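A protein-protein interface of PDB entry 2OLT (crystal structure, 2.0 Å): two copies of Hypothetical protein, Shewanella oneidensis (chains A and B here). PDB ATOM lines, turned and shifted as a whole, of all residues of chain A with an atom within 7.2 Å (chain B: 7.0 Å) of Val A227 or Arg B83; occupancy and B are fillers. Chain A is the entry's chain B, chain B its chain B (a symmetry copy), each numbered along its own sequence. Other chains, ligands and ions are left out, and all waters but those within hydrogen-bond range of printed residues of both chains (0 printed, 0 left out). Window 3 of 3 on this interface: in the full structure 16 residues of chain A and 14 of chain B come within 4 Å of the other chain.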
ATOM      1  N   PRO A  80      15.905   8.262  14.000  1.00  0.00           N
ATOM      2  CA  PRO A  80      16.456   6.946  14.373  1.00  0.00           C
ATOM      3  C   PRO A  80      16.629   5.941  13.252  1.00  0.00           C
ATOM      4  O   PRO A  80      17.148   4.857  13.505  1.00  0.00           O
ATOM      5  CB  PRO A  80      15.400   6.399  15.315  1.00  0.00           C
ATOM      6  CG  PRO A  80      14.151   6.913  14.742  1.00  0.00           C
ATOM      7  CD  PRO A  80      14.463   8.316  14.285  1.00  0.00           C
ATOM      8  N   GLU A 155      16.321  -7.285  18.054  1.00  0.00           N
ATOM      9  CA  GLU A 155      16.209  -7.234  16.580  1.00  0.00           C
ATOM     10  C   GLU A 155      16.372  -8.614  15.931  1.00  0.00           C
ATOM     11  O   GLU A 155      15.765  -8.888  14.895  1.00  0.00           O
ATOM     12  CB  GLU A 155      17.195  -6.243  15.947  1.00  0.00           C
ATOM     13  N   LEU A 222      17.045  -4.867   6.429  1.00  0.00           N
ATOM     14  CA  LEU A 222      18.253  -4.067   6.168  1.00  0.00           C
ATOM     15  C   LEU A 222      18.352  -2.881   7.125  1.00  0.00           C
ATOM     16  O   LEU A 222      19.445  -2.514   7.550  1.00  0.00           O
ATOM     17  CB  LEU A 222      18.295  -3.517   4.744  1.00  0.00           C
ATOM     18  CG  LEU A 222      18.572  -4.496   3.616  1.00  0.00           C
ATOM     19  CD1 LEU A 222      18.283  -3.856   2.244  1.00  0.00           C
ATOM     20  CD2 LEU A 222      19.977  -5.056   3.692  1.00  0.00           C
ATOM     21  N   MET A 223      17.210  -2.264   7.415  1.00  0.00           N
ATOM     22  CA  MET A 223      17.169  -1.151   8.350  1.00  0.00           C
ATOM     23  C   MET A 223      17.672  -1.608   9.701  1.00  0.00           C
ATOM     24  O   MET A 223      18.485  -0.943  10.318  1.00  0.00           O
ATOM     25  CB  MET A 223      15.752  -0.609   8.527  1.00  0.00           C
ATOM     26  CG  MET A 223      15.196   0.056   7.340  1.00  0.00           C
ATOM     27  SD  MET A 223      13.357   0.703   7.623  1.00  0.00           S
ATOM     28  CE  MET A 223      13.629   1.950   8.575  1.00  0.00           C
ATOM     29  N   LEU A 224      17.199  -2.766  10.147  1.00  0.00           N
ATOM     30  CA  LEU A 224      17.612  -3.297  11.438  1.00  0.00           C
ATOM     31  C   LEU A 224      19.074  -3.702  11.455  1.00  0.00           C
ATOM     32  O   LEU A 224      19.678  -3.687  12.502  1.00  0.00           O
ATOM     33  CB  LEU A 224      16.730  -4.481  11.842  1.00  0.00           C
ATOM     34  CG  LEU A 224      15.242  -4.155  12.044  1.00  0.00           C
ATOM     35  CD1 LEU A 224      14.400  -5.412  12.186  1.00  0.00           C
ATOM     36  CD2 LEU A 224      15.069  -3.249  13.256  1.00  0.00           C
ATOM     37  N   ALA A 225      19.652  -4.047  10.310  1.00  0.00           N
ATOM     38  CA  ALA A 225      21.066  -4.443  10.267  1.00  0.00           C
ATOM     39  C   ALA A 225      22.038  -3.271  10.251  1.00  0.00           C
ATOM     40  O   ALA A 225      23.243  -3.456  10.363  1.00  0.00           O
ATOM     41  CB  ALA A 225      21.323  -5.321   9.084  1.00  0.00           C
ATOM     42  N   ARG A 226      21.525  -2.070  10.084  1.00  0.00           N
ATOM     43  CA  ARG A 226      22.339  -0.881  10.046  1.00  0.00           C
ATOM     44  C   ARG A 226      22.643  -0.395  11.483  1.00  0.00           C
ATOM     45  O   ARG A 226      23.695   0.203  11.740  1.00  0.00           O
ATOM     46  CB  ARG A 226      21.547   0.140   9.235  1.00  0.00           C
ATOM     47  CG  ARG A 226      22.362   1.144   8.508  1.00  0.00           C
ATOM     48  CD  ARG A 226      21.587   1.729   7.353  1.00  0.00           C
ATOM     49  NE  ARG A 226      21.514   0.798   6.241  1.00  0.00           N
ATOM     50  CZ  ARG A 226      20.935   1.078   5.089  1.00  0.00           C
ATOM     51  NH1 ARG A 226      20.386   2.258   4.929  1.00  0.00           N
ATOM     52  NH2 ARG A 226      20.872   0.201   4.102  1.00  0.00           N
ATOM     53  N   VAL A 227      21.741  -0.707  12.414  1.00  0.00           N
ATOM     54  CA  VAL A 227      21.837  -0.306  13.819  1.00  0.00           C
ATOM     55  C   VAL A 227      22.947  -1.043  14.579  1.00  0.00           C
ATOM     56  O   VAL A 227      23.393  -2.123  14.163  1.00  0.00           O
ATOM     57  CB  VAL A 227      20.481  -0.553  14.550  1.00  0.00           C
ATOM     58  N   THR B  72      22.769 -14.023  12.276  1.00  0.00           N
ATOM     59  CA  THR B  72      24.109 -13.851  12.844  1.00  0.00           C
ATOM     60  C   THR B  72      24.765 -12.497  12.513  1.00  0.00           C
ATOM     61  O   THR B  72      25.227 -11.785  13.403  1.00  0.00           O
ATOM     62  CB  THR B  72      25.032 -14.956  12.326  1.00  0.00           C
ATOM     63  OG1 THR B  72      24.601 -16.209  12.853  1.00  0.00           O
ATOM     64  CG2 THR B  72      26.453 -14.712  12.773  1.00  0.00           C
ATOM     65  N   LEU B  73      24.821 -12.176  11.225  1.00  0.00           N
ATOM     66  CA  LEU B  73      25.430 -10.946  10.703  1.00  0.00           C
ATOM     67  C   LEU B  73      25.177  -9.805  11.692  1.00  0.00           C
ATOM     68  O   LEU B  73      26.144  -9.284  12.257  1.00  0.00           O
ATOM     69  CB  LEU B  73      24.899 -10.627   9.288  1.00  0.00           C
ATOM     70  CG  LEU B  73      25.839 -10.076   8.206  1.00  0.00           C
ATOM     71  N   PRO B  74      23.885  -9.440  11.951  1.00  0.00           N
ATOM     72  CA  PRO B  74      23.580  -8.367  12.938  1.00  0.00           C
ATOM     73  C   PRO B  74      24.493  -8.392  14.165  1.00  0.00           C
ATOM     74  O   PRO B  74      24.967  -7.342  14.598  1.00  0.00           O
ATOM     75  CB  PRO B  74      22.114  -8.654  13.356  1.00  0.00           C
ATOM     76  CG  PRO B  74      21.655  -9.874  12.535  1.00  0.00           C
ATOM     77  CD  PRO B  74      22.635  -9.973  11.368  1.00  0.00           C
ATOM     78  N   SER B  75      24.720  -9.580  14.731  1.00  0.00           N
ATOM     79  CA  SER B  75      25.667  -9.743  15.851  1.00  0.00           C
ATOM     80  C   SER B  75      27.156  -9.472  15.742  1.00  0.00           C
ATOM     81  O   SER B  75      27.935  -9.652  16.687  1.00  0.00           O
ATOM     82  CB  SER B  75      25.185 -10.642  17.010  1.00  0.00           C
ATOM     83  N   GLY B  76      27.531  -9.055  14.526  1.00  0.00           N
ATOM     84  CA  GLY B  76      28.902  -8.747  14.114  1.00  0.00           C
ATOM     85  C   GLY B  76      29.469  -7.470  14.703  1.00  0.00           C
ATOM     86  O   GLY B  76      28.751  -6.474  14.832  1.00  0.00           O
ATOM     87  N   LEU B  77      30.756  -7.493  15.050  1.00  0.00           N
ATOM     88  CA  LEU B  77      31.411  -6.335  15.672  1.00  0.00           C
ATOM     89  C   LEU B  77      32.207  -5.555  14.621  1.00  0.00           C
ATOM     90  O   LEU B  77      31.614  -4.982  13.704  1.00  0.00           O
ATOM     91  CB  LEU B  77      32.290  -6.758  16.866  1.00  0.00           C
ATOM     92  N   MET B  79      34.181  -5.042  11.368  1.00  0.00           N
ATOM     93  CA  MET B  79      33.997  -5.811  10.151  1.00  0.00           C
ATOM     94  C   MET B  79      34.418  -4.981   8.943  1.00  0.00           C
ATOM     95  O   MET B  79      34.076  -3.813   8.871  1.00  0.00           O
ATOM     96  CB  MET B  79      32.530  -6.204  10.042  1.00  0.00           C
ATOM     97  CG  MET B  79      32.373  -7.637   9.671  1.00  0.00           C
ATOM     98  SD  MET B  79      30.582  -8.108   9.291  1.00  0.00           S
ATOM     99  CE  MET B  79      29.789  -7.816  11.030  1.00  0.00           C
ATOM    100  N   VAL B  81      33.497  -5.061   5.767  1.00  0.00           N
ATOM    101  CA  VAL B  81      32.441  -4.799   4.783  1.00  0.00           C
ATOM    102  C   VAL B  81      31.156  -4.449   5.528  1.00  0.00           C
ATOM    103  O   VAL B  81      31.023  -4.783   6.705  1.00  0.00           O
ATOM    104  CB  VAL B  81      32.199  -6.033   3.868  1.00  0.00           C
ATOM    105  CG1 VAL B  81      33.432  -6.323   3.047  1.00  0.00           C
ATOM    106  CG2 VAL B  81      31.840  -7.267   4.686  1.00  0.00           C
ATOM    107  N   GLU B  82      30.213  -3.802   4.844  1.00  0.00           N
ATOM    108  CA  GLU B  82      28.928  -3.464   5.447  1.00  0.00           C
ATOM    109  C   GLU B  82      28.051  -4.683   5.587  1.00  0.00           C
ATOM    110  O   GLU B  82      27.923  -5.469   4.641  1.00  0.00           O
ATOM    111  CB  GLU B  82      28.181  -2.441   4.594  1.00  0.00           C
ATOM    112  CG  GLU B  82      28.913  -1.129   4.462  1.00  0.00           C
ATOM    113  CD  GLU B  82      29.068  -0.426   5.772  1.00  0.00           C
ATOM    114  OE1 GLU B  82      28.078  -0.403   6.548  1.00  0.00           O
ATOM    115  OE2 GLU B  82      30.167   0.131   6.019  1.00  0.00           O
ATOM    116  N   ARG B  83      27.453  -4.828   6.774  1.00  0.00           N
ATOM    117  CA  ARG B  83      26.474  -5.879   7.038  1.00  0.00           C
ATOM    118  C   ARG B  83      25.393  -5.834   5.982  1.00  0.00           C
ATOM    119  O   ARG B  83      24.982  -6.858   5.480  1.00  0.00           O
ATOM    120  CB  ARG B  83      25.810  -5.694   8.416  1.00  0.00           C
ATOM    121  CG  ARG B  83      26.618  -6.135   9.608  1.00  0.00           C
ATOM    122  CD  ARG B  83      25.945  -5.843  11.016  1.00  0.00           C
ATOM    123  NE  ARG B  83      26.476  -4.671  11.740  1.00  0.00           N
ATOM    124  CZ  ARG B  83      25.837  -3.515  11.943  1.00  0.00           C
ATOM    125  N   THR B  84      24.923  -4.638   5.651  1.00  0.00           N
ATOM    126  CA  THR B  84      23.852  -4.510   4.673  1.00  0.00           C
ATOM    127  C   THR B  84      24.262  -4.995   3.282  1.00  0.00           C
ATOM    128  O   THR B  84      23.446  -5.543   2.577  1.00  0.00           O
ATOM    129  CB  THR B  84      23.290  -3.088   4.630  1.00  0.00           C
ATOM    130  OG1 THR B  84      24.332  -2.139   4.354  1.00  0.00           O
ATOM    131  CG2 THR B  84      22.621  -2.737   5.965  1.00  0.00           C
ATOM    132  N   ASP B  85      25.515  -4.793   2.889  1.00  0.00           N
ATOM    133  CA  ASP B  85      25.973  -5.271   1.585  1.00  0.00           C
ATOM    134  C   ASP B  85      25.972  -6.766   1.536  1.00  0.00           C
ATOM    135  O   ASP B  85      25.615  -7.352   0.515  1.00  0.00           O
ATOM    136  CB  ASP B  85      27.370  -4.732   1.221  1.00  0.00           C
ATOM    137  CG  ASP B  85      27.346  -3.280   0.784  1.00  0.00           C
ATOM    138  OD1 ASP B  85      26.290  -2.804   0.344  1.00  0.00           O
ATOM    139  OD2 ASP B  85      28.374  -2.585   0.898  1.00  0.00           O
ATOM    140  N   LEU B  86      26.375  -7.409   2.633  1.00  0.00           N
ATOM    141  CA  LEU B  86      26.346  -8.848   2.728  1.00  0.00           C
ATOM    142  C   LEU B  86      24.921  -9.395   2.640  1.00  0.00           C
ATOM    143  O   LEU B  86      24.700 -10.429   2.011  1.00  0.00           O
ATOM    144  CB  LEU B  86      26.996  -9.318   4.046  1.00  0.00           C
ATOM    145  CG  LEU B  86      28.466  -8.938   4.210  1.00  0.00           C
ATOM    146  CD1 LEU B  86      29.040  -9.542   5.502  1.00  0.00           C
ATOM    147  CD2 LEU B  86      29.267  -9.394   3.006  1.00  0.00           C
ATOM    148  N   LEU B  87      23.964  -8.721   3.302  1.00  0.00           N
ATOM    149  CA  LEU B  87      22.577  -9.156   3.235  1.00  0.00           C
ATOM    150  C   LEU B  87      22.061  -9.015   1.816  1.00  0.00           C
ATOM    151  O   LEU B  87      21.373  -9.896   1.330  1.00  0.00           O
ATOM    152  CB  LEU B  87      21.677  -8.370   4.202  1.00  0.00           C
ATOM    153  CG  LEU B  87      21.850  -8.649   5.696  1.00  0.00           C
ATOM    154  CD1 LEU B  87      20.914  -7.766   6.520  1.00  0.00           C
ATOM    155  CD2 LEU B  87      21.609 -10.105   6.012  1.00  0.00           C
ATOM    156  N   GLU B  88      22.378  -7.895   1.155  1.00  0.00           N
ATOM    157  CA  GLU B  88      21.904  -7.662  -0.223  1.00  0.00           C
ATOM    158  C   GLU B  88      22.514  -8.681  -1.167  1.00  0.00           C
ATOM    159  O   GLU B  88      21.847  -9.210  -2.050  1.00  0.00           O
ATOM    160  CB  GLU B  88      22.143  -6.202  -0.673  1.00  0.00           C
ATOM    161  CG  GLU B  88      21.573  -5.225   0.322  1.00  0.00           C
ATOM    162  CD  GLU B  88      21.133  -3.876  -0.252  1.00  0.00           C
ATOM    163  OE1 GLU B  88      20.195  -3.884  -1.081  1.00  0.00           O
ATOM    164  OE2 GLU B  88      21.654  -2.816   0.207  1.00  0.00           O
ATOM    165  N   LEU B  89      23.780  -9.013  -0.938  1.00  0.00           N
ATOM    166  CA  LEU B  89      24.425 -10.047  -1.715  1.00  0.00           C
ATOM    167  C   LEU B  89      23.712 -11.414  -1.528  1.00  0.00           C
ATOM    168  O   LEU B  89      23.369 -12.122  -2.480  1.00  0.00           O
ATOM    169  CB  LEU B  89      25.888 -10.095  -1.303  1.00  0.00           C
ATOM    170  CG  LEU B  89      26.783 -11.038  -2.058  1.00  0.00           C
ATOM    171  CD1 LEU B  89      26.899 -10.630  -3.527  1.00  0.00           C
ATOM    172  CD2 LEU B  89      28.168 -11.078  -1.386  1.00  0.00           C
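Among the printed residues, pairs that only touch across the chains: Ala A225 with Arg B83, Leu A222 with Thr B84, Ala A225 with Leu B87, Val A227 with Arg B83, Arg A226 with Thr B84, Leu A222 with Glu B88 and Leu A222 with Leu B87.
Of chain B, only Arg B83 (3.6 Å) comes within 4 Å of Val A227. Of the printed residues of chain A, Leu B87 touches Leu A222 (3.8 Å) and Ala A225 (3.6 Å). Of the printed residues of chain B, Ala A225 touches Arg B83 (3.0 Å) and Leu B87 (3.6 Å). Leu B73 touches none of the printed residues of chain A. Thr B72 touches none of the printed residues of chain A.
Printed residues of chain B that touch a printed residue of chain A: Arg B83, Thr B84, Leu B87 and Glu B88. Among the printed residues, 7 pairs touch across the chains. Among the printed residues, no Asp or Glu carboxylate lies within 4 Å of a Lys or Arg side-chain nitrogen of the other chain.
No position is printed for both chains.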
